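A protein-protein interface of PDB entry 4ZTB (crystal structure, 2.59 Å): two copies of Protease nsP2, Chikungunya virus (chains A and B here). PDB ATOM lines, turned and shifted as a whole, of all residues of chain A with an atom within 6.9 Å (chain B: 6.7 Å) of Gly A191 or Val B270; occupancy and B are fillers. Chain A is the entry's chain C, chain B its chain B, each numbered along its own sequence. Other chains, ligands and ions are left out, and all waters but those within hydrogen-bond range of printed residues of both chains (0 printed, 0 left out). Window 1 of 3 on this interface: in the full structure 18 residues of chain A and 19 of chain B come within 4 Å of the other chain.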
ATOM      1  N   ASN A 173       1.932  28.525   5.917  1.00  0.00           N
ATOM      2  CA  ASN A 173       0.547  28.578   5.411  1.00  0.00           C
ATOM      3  C   ASN A 173      -0.304  29.635   6.101  1.00  0.00           C
ATOM      4  O   ASN A 173      -0.005  30.036   7.231  1.00  0.00           O
ATOM      5  CB  ASN A 173      -0.116  27.185   5.584  1.00  0.00           C
ATOM      6  CG  ASN A 173      -1.367  26.974   4.700  1.00  0.00           C
ATOM      7  OD1 ASN A 173      -1.547  27.618   3.649  1.00  0.00           O
ATOM      8  ND2 ASN A 173      -2.225  26.057   5.121  1.00  0.00           N
ATOM      9  N   TRP A 183      -0.994  25.801  -1.855  1.00  0.00           N
ATOM     10  CA  TRP A 183       0.221  26.291  -1.161  1.00  0.00           C
ATOM     11  C   TRP A 183       1.531  25.671  -1.698  1.00  0.00           C
ATOM     12  O   TRP A 183       1.756  24.463  -1.568  1.00  0.00           O
ATOM     13  CB  TRP A 183       0.086  26.098   0.381  1.00  0.00           C
ATOM     14  CG  TRP A 183       1.304  26.475   1.164  1.00  0.00           C
ATOM     15  CD1 TRP A 183       2.173  27.485   0.876  1.00  0.00           C
ATOM     16  CD2 TRP A 183       1.790  25.867   2.370  1.00  0.00           C
ATOM     17  NE1 TRP A 183       3.180  27.541   1.809  1.00  0.00           N
ATOM     18  CE2 TRP A 183       2.973  26.565   2.743  1.00  0.00           C
ATOM     19  CE3 TRP A 183       1.351  24.803   3.174  1.00  0.00           C
ATOM     20  CZ2 TRP A 183       3.728  26.231   3.892  1.00  0.00           C
ATOM     21  CZ3 TRP A 183       2.112  24.461   4.332  1.00  0.00           C
ATOM     22  CH2 TRP A 183       3.283  25.180   4.671  1.00  0.00           C
ATOM     23  N   VAL A 189       9.824  21.793   3.500  1.00  0.00           N
ATOM     24  CA  VAL A 189       8.617  22.224   4.218  1.00  0.00           C
ATOM     25  C   VAL A 189       7.550  21.146   3.995  1.00  0.00           C
ATOM     26  O   VAL A 189       7.329  20.709   2.857  1.00  0.00           O
ATOM     27  CB  VAL A 189       8.116  23.622   3.760  1.00  0.00           C
ATOM     28  CG1 VAL A 189       6.831  24.022   4.460  1.00  0.00           C
ATOM     29  CG2 VAL A 189       9.180  24.682   4.026  1.00  0.00           C
ATOM     30  N   ARG A 190       6.908  20.732   5.091  1.00  0.00           N
ATOM     31  CA  ARG A 190       5.843  19.733   5.107  1.00  0.00           C
ATOM     32  C   ARG A 190       4.525  20.469   5.273  1.00  0.00           C
ATOM     33  O   ARG A 190       4.493  21.609   5.776  1.00  0.00           O
ATOM     34  CB  ARG A 190       6.011  18.728   6.265  1.00  0.00           C
ATOM     35  CG  ARG A 190       7.406  18.127   6.460  1.00  0.00           C
ATOM     36  CD  ARG A 190       7.851  17.230   5.329  1.00  0.00           C
ATOM     37  NE  ARG A 190       9.306  17.009   5.393  1.00  0.00           N
ATOM     38  CZ  ARG A 190       9.944  16.102   6.146  1.00  0.00           C
ATOM     39  NH1 ARG A 190       9.287  15.269   6.948  1.00  0.00           N
ATOM     40  NH2 ARG A 190      11.279  16.024   6.096  1.00  0.00           N
ATOM     41  N   GLY A 191       3.445  19.817   4.858  1.00  0.00           N
ATOM     42  CA  GLY A 191       2.090  20.392   4.903  1.00  0.00           C
ATOM     43  C   GLY A 191       1.679  21.171   3.660  1.00  0.00           C
ATOM     44  O   GLY A 191       0.524  21.646   3.590  1.00  0.00           O
ATOM     45  N   ALA A 192       2.592  21.309   2.681  1.00  0.00           N
ATOM     46  CA  ALA A 192       2.322  22.068   1.451  1.00  0.00           C
ATOM     47  C   ALA A 192       1.847  21.174   0.336  1.00  0.00           C
ATOM     48  O   ALA A 192       2.094  19.955   0.335  1.00  0.00           O
ATOM     49  CB  ALA A 192       3.556  22.826   1.022  1.00  0.00           C
ATOM     50  N   ASP A 193       1.153  21.794  -0.614  1.00  0.00           N
ATOM     51  CA  ASP A 193       0.651  21.108  -1.802  1.00  0.00           C
ATOM     52  C   ASP A 193       1.820  20.794  -2.727  1.00  0.00           C
ATOM     53  O   ASP A 193       1.877  19.707  -3.298  1.00  0.00           O
ATOM     54  CB  ASP A 193      -0.405  21.946  -2.515  1.00  0.00           C
ATOM     55  CG  ASP A 193      -1.643  22.132  -1.677  1.00  0.00           C
ATOM     56  OD1 ASP A 193      -2.271  21.120  -1.312  1.00  0.00           O
ATOM     57  OD2 ASP A 193      -1.995  23.283  -1.378  1.00  0.00           O
ATOM     58  N   TYR A 194       2.752  21.738  -2.878  1.00  0.00           N
ATOM     59  CA  TYR A 194       3.969  21.527  -3.686  1.00  0.00           C
ATOM     60  C   TYR A 194       5.171  22.160  -3.011  1.00  0.00           C
ATOM     61  O   TYR A 194       5.025  23.116  -2.227  1.00  0.00           O
ATOM     62  CB  TYR A 194       3.802  22.109  -5.089  1.00  0.00           C
ATOM     63  CG  TYR A 194       2.643  21.527  -5.853  1.00  0.00           C
ATOM     64  CD1 TYR A 194       2.733  20.252  -6.418  1.00  0.00           C
ATOM     65  CD2 TYR A 194       1.435  22.243  -6.017  1.00  0.00           C
ATOM     66  CE1 TYR A 194       1.669  19.699  -7.126  1.00  0.00           C
ATOM     67  CE2 TYR A 194       0.358  21.690  -6.732  1.00  0.00           C
ATOM     68  CZ  TYR A 194       0.487  20.419  -7.281  1.00  0.00           C
ATOM     69  OH  TYR A 194      -0.548  19.866  -7.976  1.00  0.00           O
ATOM     70  N   THR A 195       6.354  21.611  -3.314  1.00  0.00           N
ATOM     71  CA  THR A 195       7.641  22.148  -2.844  1.00  0.00           C
ATOM     72  C   THR A 195       8.557  22.295  -4.051  1.00  0.00           C
ATOM     73  O   THR A 195       8.639  21.389  -4.896  1.00  0.00           O
ATOM     74  CB  THR A 195       8.303  21.283  -1.749  1.00  0.00           C
ATOM     75  OG1 THR A 195       8.359  19.924  -2.180  1.00  0.00           O
ATOM     76  CG2 THR A 195       7.511  21.354  -0.462  1.00  0.00           C
ATOM     77  N   GLN B 236       1.877  13.330   8.807  1.00  0.00           N
ATOM     78  CA  GLN B 236       2.483  14.547   8.236  1.00  0.00           C
ATOM     79  C   GLN B 236       3.787  14.253   7.527  1.00  0.00           C
ATOM     80  O   GLN B 236       3.993  14.651   6.375  1.00  0.00           O
ATOM     81  CB  GLN B 236       2.719  15.584   9.367  1.00  0.00           C
ATOM     82  CG  GLN B 236       3.333  16.949   9.001  1.00  0.00           C
ATOM     83  CD  GLN B 236       2.354  17.877   8.310  1.00  0.00           C
ATOM     84  OE1 GLN B 236       1.833  18.823   8.936  1.00  0.00           O
ATOM     85  NE2 GLN B 236       2.073  17.624   7.030  1.00  0.00           N
ATOM     86  N   GLY B 240       3.249  12.638   3.800  1.00  0.00           N
ATOM     87  CA  GLY B 240       3.663  13.768   2.955  1.00  0.00           C
ATOM     88  C   GLY B 240       4.878  13.447   2.122  1.00  0.00           C
ATOM     89  O   GLY B 240       4.883  13.693   0.915  1.00  0.00           O
ATOM     90  N   LEU B 243       4.668  11.341  -1.174  1.00  0.00           N
ATOM     91  CA  LEU B 243       4.238  12.005  -2.444  1.00  0.00           C
ATOM     92  C   LEU B 243       5.349  12.073  -3.531  1.00  0.00           C
ATOM     93  O   LEU B 243       5.038  11.987  -4.728  1.00  0.00           O
ATOM     94  CB  LEU B 243       3.655  13.408  -2.159  1.00  0.00           C
ATOM     95  CG  LEU B 243       2.418  13.513  -1.228  1.00  0.00           C
ATOM     96  CD1 LEU B 243       2.016  14.966  -1.023  1.00  0.00           C
ATOM     97  CD2 LEU B 243       1.238  12.714  -1.758  1.00  0.00           C
ATOM     98  N   GLU B 265      -6.533  15.797  10.118  1.00  0.00           N
ATOM     99  CA  GLU B 265      -7.492  16.181   9.059  1.00  0.00           C
ATOM    100  C   GLU B 265      -6.865  17.106   7.976  1.00  0.00           C
ATOM    101  O   GLU B 265      -7.254  17.004   6.803  1.00  0.00           O
ATOM    102  CB  GLU B 265      -8.773  16.804   9.651  1.00  0.00           C
ATOM    103  CG  GLU B 265      -9.842  17.124   8.589  1.00  0.00           C
ATOM    104  CD  GLU B 265     -11.242  17.358   9.138  1.00  0.00           C
ATOM    105  OE1 GLU B 265     -11.400  17.596  10.349  1.00  0.00           O
ATOM    106  OE2 GLU B 265     -12.194  17.302   8.335  1.00  0.00           O
ATOM    107  N   ARG B 266      -5.920  17.986   8.362  1.00  0.00           N
ATOM    108  CA  ARG B 266      -5.209  18.862   7.401  1.00  0.00           C
ATOM    109  C   ARG B 266      -4.362  18.040   6.446  1.00  0.00           C
ATOM    110  O   ARG B 266      -4.414  18.263   5.218  1.00  0.00           O
ATOM    111  CB  ARG B 266      -4.298  19.937   8.081  1.00  0.00           C
ATOM    112  CG  ARG B 266      -4.930  21.146   8.858  1.00  0.00           C
ATOM    113  CD  ARG B 266      -6.191  21.753   8.206  1.00  0.00           C
ATOM    114  NE  ARG B 266      -7.125  22.494   9.189  1.00  0.00           N
ATOM    115  CZ  ARG B 266      -6.815  23.593   9.921  1.00  0.00           C
ATOM    116  NH1 ARG B 266      -5.600  24.162   9.866  1.00  0.00           N
ATOM    117  NH2 ARG B 266      -7.749  24.146  10.754  1.00  0.00           N
ATOM    118  N   VAL B 267      -3.590  17.100   7.006  1.00  0.00           N
ATOM    119  CA  VAL B 267      -2.712  16.212   6.218  1.00  0.00           C
ATOM    120  C   VAL B 267      -3.528  15.457   5.168  1.00  0.00           C
ATOM    121  O   VAL B 267      -3.170  15.448   3.996  1.00  0.00           O
ATOM    122  CB  VAL B 267      -1.928  15.200   7.098  1.00  0.00           C
ATOM    123  CG1 VAL B 267      -1.171  14.174   6.236  1.00  0.00           C
ATOM    124  CG2 VAL B 267      -0.957  15.926   8.038  1.00  0.00           C
ATOM    125  N   ILE B 268      -4.626  14.847   5.608  1.00  0.00           N
ATOM    126  CA  ILE B 268      -5.509  14.063   4.723  1.00  0.00           C
ATOM    127  C   ILE B 268      -6.087  14.931   3.582  1.00  0.00           C
ATOM    128  O   ILE B 268      -6.214  14.436   2.454  1.00  0.00           O
ATOM    129  CB  ILE B 268      -6.610  13.318   5.533  1.00  0.00           C
ATOM    130  CG1 ILE B 268      -5.982  12.323   6.544  1.00  0.00           C
ATOM    131  CG2 ILE B 268      -7.583  12.575   4.622  1.00  0.00           C
ATOM    132  CD1 ILE B 268      -5.039  11.285   5.970  1.00  0.00           C
ATOM    133  N   CYS B 269      -6.424  16.194   3.872  1.00  0.00           N
ATOM    134  CA  CYS B 269      -6.901  17.129   2.825  1.00  0.00           C
ATOM    135  C   CYS B 269      -5.787  17.445   1.808  1.00  0.00           C
ATOM    136  O   CYS B 269      -6.064  17.529   0.609  1.00  0.00           O
ATOM    137  CB  CYS B 269      -7.473  18.420   3.418  1.00  0.00           C
ATOM    138  SG  CYS B 269      -9.027  18.180   4.299  1.00  0.00           S
ATOM    139  N   VAL B 270      -4.548  17.612   2.281  1.00  0.00           N
ATOM    140  CA  VAL B 270      -3.388  17.857   1.385  1.00  0.00           C
ATOM    141  C   VAL B 270      -3.147  16.643   0.473  1.00  0.00           C
ATOM    142  O   VAL B 270      -2.971  16.813  -0.732  1.00  0.00           O
ATOM    143  CB  VAL B 270      -2.093  18.250   2.178  1.00  0.00           C
ATOM    144  CG1 VAL B 270      -0.841  18.270   1.287  1.00  0.00           C
ATOM    145  CG2 VAL B 270      -2.275  19.612   2.856  1.00  0.00           C
ATOM    146  N   LEU B 271      -3.153  15.438   1.063  1.00  0.00           N
ATOM    147  CA  LEU B 271      -2.935  14.179   0.324  1.00  0.00           C
ATOM    148  C   LEU B 271      -4.058  13.886  -0.675  1.00  0.00           C
ATOM    149  O   LEU B 271      -3.785  13.600  -1.838  1.00  0.00           O
ATOM    150  CB  LEU B 271      -2.777  12.985   1.282  1.00  0.00           C
ATOM    151  CG  LEU B 271      -1.634  12.977   2.298  1.00  0.00           C
ATOM    152  CD1 LEU B 271      -1.687  11.683   3.102  1.00  0.00           C
ATOM    153  CD2 LEU B 271      -0.267  13.140   1.648  1.00  0.00           C
ATOM    154  N   GLY B 272      -5.311  13.965  -0.211  1.00  0.00           N
ATOM    155  CA  GLY B 272      -6.522  13.723  -1.051  1.00  0.00           C
ATOM    156  C   GLY B 272      -6.641  14.472  -2.385  1.00  0.00           C
ATOM    157  O   GLY B 272      -7.272  13.982  -3.315  1.00  0.00           O
ATOM    158  N   ARG B 273      -6.027  15.651  -2.467  1.00  0.00           N
ATOM    159  CA  ARG B 273      -6.001  16.465  -3.697  1.00  0.00           C
ATOM    160  C   ARG B 273      -5.143  15.892  -4.840  1.00  0.00           C
ATOM    161  O   ARG B 273      -5.316  16.308  -5.989  1.00  0.00           O
ATOM    162  CB  ARG B 273      -5.468  17.874  -3.375  1.00  0.00           C
ATOM    163  CG  ARG B 273      -6.335  18.709  -2.440  1.00  0.00           C
ATOM    164  CD  ARG B 273      -5.496  19.710  -1.662  1.00  0.00           C
ATOM    165  NE  ARG B 273      -6.294  20.645  -0.854  1.00  0.00           N
ATOM    166  CZ  ARG B 273      -5.792  21.553  -0.003  1.00  0.00           C
ATOM    167  NH1 ARG B 273      -4.469  21.680   0.188  1.00  0.00           N
ATOM    168  NH2 ARG B 273      -6.625  22.350   0.676  1.00  0.00           N
ATOM    169  N   LYS B 274      -4.222  14.964  -4.536  1.00  0.00           N
ATOM    170  CA  LYS B 274      -3.271  14.410  -5.539  1.00  0.00           C
ATOM    171  C   LYS B 274      -3.609  13.059  -6.161  1.00  0.00           C
ATOM    172  O   LYS B 274      -2.875  12.598  -7.057  1.00  0.00           O
ATOM    173  CB  LYS B 274      -1.879  14.305  -4.893  1.00  0.00           C
ATOM    174  CG  LYS B 274      -1.443  15.612  -4.238  1.00  0.00           C
ATOM    175  CD  LYS B 274       0.052  15.788  -4.234  1.00  0.00           C
ATOM    176  CE  LYS B 274       0.434  17.132  -3.672  1.00  0.00           C
ATOM    177  NZ  LYS B 274      -0.136  18.276  -4.462  1.00  0.00           N
ATOM    178  N   PHE B 275      -4.698  12.437  -5.697  1.00  0.00           N
ATOM    179  CA  PHE B 275      -5.130  11.113  -6.126  1.00  0.00           C
ATOM    180  C   PHE B 275      -6.528  11.179  -6.729  1.00  0.00           C
ATOM    181  O   PHE B 275      -7.347  12.005  -6.298  1.00  0.00           O
ATOM    182  CB  PHE B 275      -5.131  10.175  -4.929  1.00  0.00           C
ATOM    183  CG  PHE B 275      -3.772   9.948  -4.321  1.00  0.00           C
ATOM    184  CD1 PHE B 275      -3.278  10.822  -3.380  1.00  0.00           C
ATOM    185  CD2 PHE B 275      -2.991   8.846  -4.686  1.00  0.00           C
ATOM    186  CE1 PHE B 275      -2.028  10.629  -2.802  1.00  0.00           C
ATOM    187  CE2 PHE B 275      -1.738   8.641  -4.118  1.00  0.00           C
ATOM    188  CZ  PHE B 275      -1.256   9.533  -3.175  1.00  0.00           C
ATOM    189  N   GLY B 302      -1.782  16.141  -8.683  1.00  0.00           N
ATOM    190  CA  GLY B 302      -2.650  17.237  -9.028  1.00  0.00           C
ATOM    191  C   GLY B 302      -3.100  18.012  -7.826  1.00  0.00           C
ATOM    192  O   GLY B 302      -2.540  17.881  -6.723  1.00  0.00           O
ATOM    193  N   ARG B 303      -4.117  18.835  -8.061  1.00  0.00           N
ATOM    194  CA  ARG B 303      -4.737  19.651  -7.040  1.00  0.00           C
ATOM    195  C   ARG B 303      -6.186  19.775  -7.430  1.00  0.00           C
ATOM    196  O   ARG B 303      -6.565  20.701  -8.145  1.00  0.00           O
ATOM    197  CB  ARG B 303      -4.031  21.021  -6.915  1.00  0.00           C
ATOM    198  CG  ARG B 303      -4.695  22.064  -5.992  1.00  0.00           C
ATOM    199  CD  ARG B 303      -4.981  21.551  -4.592  1.00  0.00           C
ATOM    200  NE  ARG B 303      -5.634  22.530  -3.695  1.00  0.00           N
ATOM    201  CZ  ARG B 303      -6.957  22.739  -3.557  1.00  0.00           C
ATOM    202  NH1 ARG B 303      -7.870  22.053  -4.262  1.00  0.00           N
ATOM    203  NH2 ARG B 303      -7.383  23.667  -2.686  1.00  0.00           N
ATOM    204  N   PHE B 306     -11.163  18.524  -2.860  1.00  0.00           N
ATOM    205  CA  PHE B 306     -11.277  17.374  -1.971  1.00  0.00           C
ATOM    206  C   PHE B 306     -11.781  17.796  -0.609  1.00  0.00           C
ATOM    207  O   PHE B 306     -11.211  18.705   0.007  1.00  0.00           O
ATOM    208  CB  PHE B 306      -9.936  16.664  -1.820  1.00  0.00           C
ATOM    209  CG  PHE B 306      -9.957  15.537  -0.816  1.00  0.00           C
ATOM    210  CD1 PHE B 306      -9.664  15.781   0.539  1.00  0.00           C
ATOM    211  CD2 PHE B 306     -10.271  14.237  -1.209  1.00  0.00           C
ATOM    212  CE1 PHE B 306      -9.686  14.749   1.479  1.00  0.00           C
ATOM    213  CE2 PHE B 306     -10.293  13.197  -0.273  1.00  0.00           C
ATOM    214  CZ  PHE B 306     -10.000  13.453   1.075  1.00  0.00           C
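Among the printed residues, merely in contact across the chains: Gly A191 with Val B270 (3.5 Å), Ala A192 with Val B270 (3.5 Å), Tyr A194 with Lys B274 (3.5 Å) and Tyr A194 with Arg B303 (3.7 Å).
No position is printed for both chains. Of the 8 pairs that touch across the chains among the printed residues, none has its exchanged pair printed and touching as well.
Gly A191 touches just these residues of chain B: Gln B236 (3.4 Å) and Val B270 (3.5 Å). Printed residues of chain B within 4 Å of Asp A193: Arg B273 (2.7 Å) and Lys B274 (2.7 Å). Thr A195 touches none of the printed residues of chain B. Of the printed residues of chain A, Gln B236 touches Gly A191 (3.4 Å). Val B270 touches two residues of chain A. Gly B272 touches none of the printed residues of chain A. Of the printed residues of chain A, Arg B303 touches Tyr A194. The nearest residue of chain A that does not touch Val B270 is Asp A193 (4.1 Å).
The backbone carbonyl oxygen of Cys B269 lies close to the guanidinium group of Arg B273 (3.5 Å). The backbone carbonyl oxygen of Arg B273 lies within hydrogen-bond range of the backbone NH of Arg B303, at 3.5 Å. The backbone NH of Trp A183 sits at hydrogen-bond distance from the side-chain carboxylate of Asp A193 (2.8 Å). NZ of Lys B274 is in hydrogen-bond range of O of Gly B302 (3.3 Å). The backbone carbonyl oxygen (O) of Trp A183 is in hydrogen-bond range of the backbone NH (N) of Tyr A194 (3.2 Å).
The side-chain hydroxyl (OH) of Tyr A194 is in hydrogen-bond range of the backbone carbonyl oxygen (O) of Gly B302. The backbone NH (N) of Gly A191 lies close to the side-chain amide nitrogen (NE2) of Gln B236, 3.4 Å away. The side-chain amino group (NZ) of Lys B274 sits at hydrogen-bond distance from the backbone carbonyl oxygen (O) of Asp A193 (2.7 Å). NH1 of Arg B273 lies within salt-bridge range of OD1 of Asp A193, 2.7 Å away.
Printed residues of chain A that touch a printed residue of chain B: Gly A191, Ala A192, Asp A193 and Tyr A194. Hydrophobic or aromatic side chains of chain A that line the printed part of chain B: Tyr A194. Of the 17 printed residues of chain B, 6 touch a printed residue of chain A. Hydrophobic or aromatic side chains of chain B within 4 Å of the printed part of chain A: Val B270. Among the printed residues, 8 pairs touch across the chains.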
